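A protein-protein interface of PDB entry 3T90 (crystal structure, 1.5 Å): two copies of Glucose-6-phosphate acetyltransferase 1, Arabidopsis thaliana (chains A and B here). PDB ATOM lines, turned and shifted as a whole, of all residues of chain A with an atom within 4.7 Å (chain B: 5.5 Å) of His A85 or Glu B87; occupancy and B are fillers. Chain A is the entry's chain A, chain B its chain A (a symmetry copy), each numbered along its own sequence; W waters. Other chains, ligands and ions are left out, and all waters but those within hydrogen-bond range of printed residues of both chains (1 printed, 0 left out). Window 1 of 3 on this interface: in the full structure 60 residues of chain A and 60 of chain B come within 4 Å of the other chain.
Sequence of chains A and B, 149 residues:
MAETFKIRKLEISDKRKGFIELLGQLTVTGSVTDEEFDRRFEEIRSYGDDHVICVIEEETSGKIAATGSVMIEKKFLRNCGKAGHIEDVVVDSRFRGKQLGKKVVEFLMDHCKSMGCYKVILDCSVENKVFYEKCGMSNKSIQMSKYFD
A ring nitrogen (NE2) of His A85 sits at hydrogen-bond distance from the side-chain carboxylate (OE2) of Glu A73 (2.7 Å). The backbone NH of Glu A73 is in hydrogen-bond range of the backbone carbonyl oxygen of Ala A83, at 2.8 Å. The backbone NH (N) of His B85 lies within hydrogen-bond range of the backbone carbonyl oxygen (O) of Met B71, 2.8 Å away. O of Met A71 sits at hydrogen-bond distance from N of His A85 (2.8 Å). OE1 of Glu A73 is in salt-bridge range of NZ of Lys A75. The backbone NH of Ser B69 is in hydrogen-bond range of the backbone carbonyl oxygen of Glu B87 (2.8 Å).
Among the printed residues, pairs that only touch across the chains: Met A71 with Met B71 (2.8 Å), His A85 with Glu B87 (3.0 Å), Glu A87 with His B85 (3.0 Å), Glu A73 with Glu B87 (3.4 Å) and Glu A73 with Met B71 (3.5 Å).
Met B71 touches its own counterpart, Met A71. His A85 touches Glu B87, and with the chains exchanged Glu A87 touches His B85. Positions printed for both chains: 69, 70, 71, 85, 86 and 87. Of the 7 pairs that touch across the chains among the printed residues, 3 have their exchanged pair printed and touching as well.
Printed residues of chain B that touch a printed residue of chain A: Met B71, His B85, Glu B87 and Asp B88. Hydrophobic or aromatic side chains of chain B that line the printed part of chain A: Met B71 and His B85. Along chain B the printed residues that touch a printed residue of chain A span positions 71 to 88. Among the printed residues, 7 pairs touch across the chains. Among the printed residues, Asp or Glu carboxylates within 4 Å of a Lys or Arg side-chain nitrogen of the other chain: Lys A75 with Glu B87 (2.9 Å) and Lys A75 with Asp B88 (2.8 Å).
The side-chain amino group of Lys A75 is in salt-bridge range of the side-chain carboxylate of Asp B88 (2.8 Å). NZ of Lys A75 lies within salt-bridge range of OE1 of Glu B87 (2.9 Å).
Water W1 lies within hydrogen-bond range of the side-chain carboxylate (OE1) of Glu A73 (3.1 Å) and the backbone NH (N) of Met B71 (3.4 Å).
Of chain A, only Glu A73 (3.4 Å), Lys A75 (2.9 Å) and His A85 (3.0 Å) come within 4 Å of Glu B87. Of the printed residues of chain A, Asp B88 touches Lys A75. Of the printed residues of chain B, Glu A87 touches His B85. Printed residues of chain A within 4 Å of His B85: Glu A87. Printed residues of chain B within 4 Å of Lys A75: Glu B87 and Asp B88. Val B89 touches none of the printed residues of chain A. Asp B123 touches none of the printed residues of chain A. The nearest residue of chain B that does not touch His A85 is Met B71 (4.2 Å).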
ATOM      1  N   SER A  69       1.294  21.765  21.775  1.00  0.00           N
ATOM      2  CA  SER A  69       0.316  21.843  20.687  1.00  0.00           C
ATOM      3  C   SER A  69      -0.391  23.189  20.660  1.00  0.00           C
ATOM      4  O   SER A  69      -0.481  23.862  21.703  1.00  0.00           O
ATOM      5  CB  SER A  69      -0.767  20.780  20.893  1.00  0.00           C
ATOM      6  OG  SER A  69      -0.186  19.485  21.011  1.00  0.00           O
ATOM      7  N   VAL A  70      -0.895  23.584  19.501  1.00  0.00           N
ATOM      8  CA  VAL A  70      -1.879  24.711  19.532  1.00  0.00           C
ATOM      9  C   VAL A  70      -3.031  24.479  18.576  1.00  0.00           C
ATOM     10  O   VAL A  70      -2.827  24.007  17.463  1.00  0.00           O
ATOM     11  CB  VAL A  70      -1.096  26.069  19.251  1.00  0.00           C
ATOM     12  CG1 VAL A  70      -0.542  26.146  17.788  1.00  0.00           C
ATOM     13  CG2 VAL A  70      -2.052  27.252  19.563  1.00  0.00           C
ATOM     14  N   MET A  71      -4.230  24.792  19.025  1.00  0.00           N
ATOM     15  CA  MET A  71      -5.424  24.681  18.241  1.00  0.00           C
ATOM     16  C   MET A  71      -5.998  26.060  18.086  1.00  0.00           C
ATOM     17  O   MET A  71      -6.219  26.756  19.132  1.00  0.00           O
ATOM     18  CB  MET A  71      -6.411  23.734  18.905  1.00  0.00           C
ATOM     19  CG  MET A  71      -7.578  23.608  17.974  1.00  0.00           C
ATOM     20  SD  MET A  71      -8.705  22.320  18.566  1.00  0.00           S
ATOM     21  CE  MET A  71      -9.373  23.057  19.740  1.00  0.00           C
ATOM     22  N   GLU A  73      -8.846  28.621  17.258  1.00  0.00           N
ATOM     23  CA  GLU A  73     -10.325  28.733  17.380  1.00  0.00           C
ATOM     24  C   GLU A  73     -10.780  29.975  16.610  1.00  0.00           C
ATOM     25  O   GLU A  73     -10.345  31.076  16.971  1.00  0.00           O
ATOM     26  CB  GLU A  73     -10.670  28.939  18.829  1.00  0.00           C
ATOM     27  CG  GLU A  73     -12.244  29.049  19.006  1.00  0.00           C
ATOM     28  CD  GLU A  73     -12.591  29.700  20.305  1.00  0.00           C
ATOM     29  OE1 GLU A  73     -13.751  30.114  20.524  1.00  0.00           O
ATOM     30  OE2 GLU A  73     -11.743  29.912  21.195  1.00  0.00           O
ATOM     31  N   LYS A  75     -13.572  32.760  15.943  1.00  0.00           N
ATOM     32  CA  LYS A  75     -14.647  33.383  16.731  1.00  0.00           C
ATOM     33  C   LYS A  75     -15.406  34.395  15.933  1.00  0.00           C
ATOM     34  O   LYS A  75     -14.963  34.711  14.776  1.00  0.00           O
ATOM     35  CB  LYS A  75     -14.020  34.106  17.938  1.00  0.00           C
ATOM     36  CG  LYS A  75     -13.294  33.170  18.909  1.00  0.00           C
ATOM     37  CD  LYS A  75     -12.827  34.011  20.078  1.00  0.00           C
ATOM     38  CE  LYS A  75     -12.189  33.243  21.238  1.00  0.00           C
ATOM     39  NZ  LYS A  75     -13.220  32.424  21.990  1.00  0.00           N
ATOM     40  N   ALA A  83      -8.230  32.851  18.016  1.00  0.00           N
ATOM     41  CA  ALA A  83      -7.434  32.687  19.227  1.00  0.00           C
ATOM     42  C   ALA A  83      -6.713  31.370  19.208  1.00  0.00           C
ATOM     43  O   ALA A  83      -7.370  30.312  18.974  1.00  0.00           O
ATOM     44  CB  ALA A  83      -8.365  32.735  20.482  1.00  0.00           C
ATOM     45  N   GLY A  84      -5.469  31.367  19.663  1.00  0.00           N
ATOM     46  CA  GLY A  84      -4.686  30.108  19.761  1.00  0.00           C
ATOM     47  C   GLY A  84      -4.823  29.544  21.157  1.00  0.00           C
ATOM     48  O   GLY A  84      -4.669  30.266  22.132  1.00  0.00           O
ATOM     49  N   HIS A  85      -5.126  28.256  21.260  1.00  0.00           N
ATOM     50  CA  HIS A  85      -5.188  27.536  22.562  1.00  0.00           C
ATOM     51  C   HIS A  85      -3.979  26.605  22.647  1.00  0.00           C
ATOM     52  O   HIS A  85      -3.940  25.575  21.922  1.00  0.00           O
ATOM     53  CB  HIS A  85      -6.463  26.682  22.588  1.00  0.00           C
ATOM     54  CG  HIS A  85      -7.731  27.483  22.497  1.00  0.00           C
ATOM     55  ND1 HIS A  85      -8.378  27.899  23.643  1.00  0.00           N
ATOM     56  CD2 HIS A  85      -8.365  28.062  21.466  1.00  0.00           C
ATOM     57  CE1 HIS A  85      -9.441  28.632  23.302  1.00  0.00           C
ATOM     58  NE2 HIS A  85      -9.466  28.751  21.983  1.00  0.00           N
ATOM     59  N   ILE A  86      -2.958  26.957  23.422  1.00  0.00           N
ATOM     60  CA  ILE A  86      -1.737  26.120  23.561  1.00  0.00           C
ATOM     61  C   ILE A  86      -2.114  25.075  24.637  1.00  0.00           C
ATOM     62  O   ILE A  86      -2.719  25.348  25.707  1.00  0.00           O
ATOM     63  CB  ILE A  86      -0.559  26.933  23.996  1.00  0.00           C
ATOM     64  CG1 ILE A  86      -0.023  27.710  22.790  1.00  0.00           C
ATOM     65  CG2 ILE A  86       0.526  26.071  24.599  1.00  0.00           C
ATOM     66  CD1 ILE A  86       1.047  28.730  23.092  1.00  0.00           C
ATOM     67  N   GLU A  87      -1.805  23.841  24.274  1.00  0.00           N
ATOM     68  CA  GLU A  87      -2.164  22.611  25.049  1.00  0.00           C
ATOM     69  C   GLU A  87      -1.010  21.624  25.112  1.00  0.00           C
ATOM     70  O   GLU A  87      -0.106  21.654  24.253  1.00  0.00           O
ATOM     71  CB  GLU A  87      -3.333  21.866  24.370  1.00  0.00           C
ATOM     72  CG  GLU A  87      -4.624  22.687  24.448  1.00  0.00           C
ATOM     73  CD  GLU A  87      -5.290  22.597  25.786  1.00  0.00           C
ATOM     74  OE1 GLU A  87      -5.171  21.543  26.522  1.00  0.00           O
ATOM     75  OE2 GLU A  87      -6.002  23.563  26.195  1.00  0.00           O
ATOM     76  N   ILE A 121      -3.715  31.614  24.483  1.00  0.00           N
ATOM     77  CA  ILE A 121      -3.942  31.249  25.860  1.00  0.00           C
ATOM     78  C   ILE A 121      -3.572  29.856  26.172  1.00  0.00           C
ATOM     79  O   ILE A 121      -3.542  29.009  25.287  1.00  0.00           O
ATOM     80  CB  ILE A 121      -5.415  31.538  26.203  1.00  0.00           C
ATOM     81  CG1 ILE A 121      -6.432  30.773  25.259  1.00  0.00           C
ATOM     82  CG2 ILE A 121      -5.710  33.049  26.112  1.00  0.00           C
ATOM     83  CD1 ILE A 121      -7.932  30.998  25.663  1.00  0.00           C
ATOM     84  N   GLY B  68     -23.084  30.833  24.189  1.00  0.00           N
ATOM     85  CA  GLY B  68     -21.824  30.211  24.621  1.00  0.00           C
ATOM     86  C   GLY B  68     -21.475  29.230  23.548  1.00  0.00           C
ATOM     87  O   GLY B  68     -22.311  28.695  22.831  1.00  0.00           O
ATOM     88  N   SER B  69     -20.182  28.955  23.437  1.00  0.00           N
ATOM     89  CA  SER B  69     -19.626  28.114  22.374  1.00  0.00           C
ATOM     90  C   SER B  69     -18.815  26.958  22.937  1.00  0.00           C
ATOM     91  O   SER B  69     -18.298  27.056  24.066  1.00  0.00           O
ATOM     92  CB  SER B  69     -18.673  28.943  21.509  1.00  0.00           C
ATOM     93  OG  SER B  69     -19.331  30.099  21.000  1.00  0.00           O
ATOM     94  N   VAL B  70     -18.687  25.881  22.177  1.00  0.00           N
ATOM     95  CA  VAL B  70     -17.622  24.900  22.555  1.00  0.00           C
ATOM     96  C   VAL B  70     -16.897  24.361  21.339  1.00  0.00           C
ATOM     97  O   VAL B  70     -17.518  24.076  20.322  1.00  0.00           O
ATOM     98  CB  VAL B  70     -18.286  23.758  23.445  1.00  0.00           C
ATOM     99  CG1 VAL B  70     -19.287  22.872  22.629  1.00  0.00           C
ATOM    100  CG2 VAL B  70     -17.147  22.907  24.068  1.00  0.00           C
ATOM    101  N   MET B  71     -15.589  24.245  21.448  1.00  0.00           N
ATOM    102  CA  MET B  71     -14.751  23.711  20.416  1.00  0.00           C
ATOM    103  C   MET B  71     -14.102  22.468  20.952  1.00  0.00           C
ATOM    104  O   MET B  71     -13.459  22.534  22.052  1.00  0.00           O
ATOM    105  CB  MET B  71     -13.719  24.740  19.982  1.00  0.00           C
ATOM    106  CG  MET B  71     -12.958  24.132  18.844  1.00  0.00           C
ATOM    107  SD  MET B  71     -11.859  25.368  18.103  1.00  0.00           S
ATOM    108  CE  MET B  71     -10.752  25.426  19.170  1.00  0.00           C
ATOM    109  N   HIS B  85     -13.584  22.787  24.862  1.00  0.00           N
ATOM    110  CA  HIS B  85     -13.174  24.138  25.335  1.00  0.00           C
ATOM    111  C   HIS B  85     -14.385  25.064  25.237  1.00  0.00           C
ATOM    112  O   HIS B  85     -14.789  25.433  24.101  1.00  0.00           O
ATOM    113  CB  HIS B  85     -12.076  24.670  24.403  1.00  0.00           C
ATOM    114  CG  HIS B  85     -10.827  23.836  24.399  1.00  0.00           C
ATOM    115  ND1 HIS B  85      -9.786  24.131  25.257  1.00  0.00           N
ATOM    116  CD2 HIS B  85     -10.513  22.677  23.799  1.00  0.00           C
ATOM    117  CE1 HIS B  85      -8.822  23.221  25.101  1.00  0.00           C
ATOM    118  NE2 HIS B  85      -9.228  22.321  24.220  1.00  0.00           N
ATOM    119  N   ILE B  86     -15.035  25.382  26.351  1.00  0.00           N
ATOM    120  CA  ILE B  86     -16.229  26.269  26.352  1.00  0.00           C
ATOM    121  C   ILE B  86     -15.640  27.699  26.359  1.00  0.00           C
ATOM    122  O   ILE B  86     -14.681  28.065  27.090  1.00  0.00           O
ATOM    123  CB  ILE B  86     -17.085  26.038  27.556  1.00  0.00           C
ATOM    124  CG1 ILE B  86     -17.899  24.759  27.346  1.00  0.00           C
ATOM    125  CG2 ILE B  86     -17.998  27.212  27.829  1.00  0.00           C
ATOM    126  CD1 ILE B  86     -18.675  24.271  28.545  1.00  0.00           C
ATOM    127  N   GLU B  87     -16.198  28.482  25.451  1.00  0.00           N
ATOM    128  CA  GLU B  87     -15.748  29.875  25.135  1.00  0.00           C
ATOM    129  C   GLU B  87     -16.923  30.824  24.968  1.00  0.00           C
ATOM    130  O   GLU B  87     -18.054  30.386  24.675  1.00  0.00           O
ATOM    131  CB  GLU B  87     -14.975  29.905  23.800  1.00  0.00           C
ATOM    132  CG  GLU B  87     -13.645  29.154  23.922  1.00  0.00           C
ATOM    133  CD  GLU B  87     -12.583  29.961  24.602  1.00  0.00           C
ATOM    134  OE1 GLU B  87     -12.571  31.250  24.528  1.00  0.00           O
ATOM    135  OE2 GLU B  87     -11.664  29.368  25.245  1.00  0.00           O
ATOM    136  N   ASP B  88     -16.677  32.118  25.119  1.00  0.00           N
ATOM    137  CA  ASP B  88     -17.602  33.155  24.641  1.00  0.00           C
ATOM    138  C   ASP B  88     -18.990  33.036  25.246  1.00  0.00           C
ATOM    139  O   ASP B  88     -20.029  33.148  24.567  1.00  0.00           O
ATOM    140  CB  ASP B  88     -17.611  33.190  23.096  1.00  0.00           C
ATOM    141  CG  ASP B  88     -16.242  33.490  22.449  1.00  0.00           C
ATOM    142  OD1 ASP B  88     -15.307  33.855  23.231  1.00  0.00           O
ATOM    143  OD2 ASP B  88     -16.156  33.323  21.252  1.00  0.00           O
ATOM    144  N   VAL B  89     -18.993  32.732  26.544  1.00  0.00           N
ATOM    145  CA  VAL B  89     -20.250  32.675  27.357  1.00  0.00           C
ATOM    146  C   VAL B  89     -20.654  34.059  27.847  1.00  0.00           C
ATOM    147  O   VAL B  89     -19.887  34.755  28.477  1.00  0.00           O
ATOM    148  CB  VAL B  89     -20.040  31.737  28.530  1.00  0.00           C
ATOM    149  CG1 VAL B  89     -21.351  31.716  29.368  1.00  0.00           C
ATOM    150  CG2 VAL B  89     -19.714  30.260  28.070  1.00  0.00           C
ATOM    151  N   LEU B 108     -23.853  22.953  26.460  1.00  0.00           N
ATOM    152  CA  LEU B 108     -22.569  22.612  25.901  1.00  0.00           C
ATOM    153  C   LEU B 108     -21.908  21.434  26.597  1.00  0.00           C
ATOM    154  O   LEU B 108     -21.255  20.657  25.881  1.00  0.00           O
ATOM    155  CB  LEU B 108     -21.695  23.859  26.033  1.00  0.00           C
ATOM    156  CG  LEU B 108     -22.240  25.132  25.354  1.00  0.00           C
ATOM    157  CD1 LEU B 108     -21.455  26.393  25.756  1.00  0.00           C
ATOM    158  CD2 LEU B 108     -22.138  24.985  23.824  1.00  0.00           C
ATOM    159  N   LEU B 122     -13.009  25.692  30.746  1.00  0.00           N
ATOM    160  CA  LEU B 122     -13.268  27.102  30.329  1.00  0.00           C
ATOM    161  C   LEU B 122     -12.471  27.984  31.251  1.00  0.00           C
ATOM    162  O   LEU B 122     -11.919  27.530  32.265  1.00  0.00           O
ATOM    163  CB  LEU B 122     -14.744  27.473  30.361  1.00  0.00           C
ATOM    164  CG  LEU B 122     -15.471  27.355  31.742  1.00  0.00           C
ATOM    165  CD1 LEU B 122     -15.202  28.584  32.649  1.00  0.00           C
ATOM    166  CD2 LEU B 122     -17.025  27.075  31.475  1.00  0.00           C
ATOM    167  N   ASP B 123     -12.336  29.245  30.877  1.00  0.00           N
ATOM    168  CA  ASP B 123     -11.681  30.250  31.757  1.00  0.00           C
ATOM    169  C   ASP B 123     -12.674  31.330  32.147  1.00  0.00           C
ATOM    170  O   ASP B 123     -13.583  31.679  31.378  1.00  0.00           O
ATOM    171  CB  ASP B 123     -10.439  30.819  31.047  1.00  0.00           C
ATOM    172  CG  ASP B 123      -9.444  29.759  30.604  1.00  0.00           C
ATOM    173  OD1 ASP B 123      -8.787  29.165  31.460  1.00  0.00           O
ATOM    174  OD2 ASP B 123      -9.159  29.633  29.389  1.00  0.00           O
HETATM  175  O   HOH W   1     -15.467  27.599  21.236  1.00  0.00           O
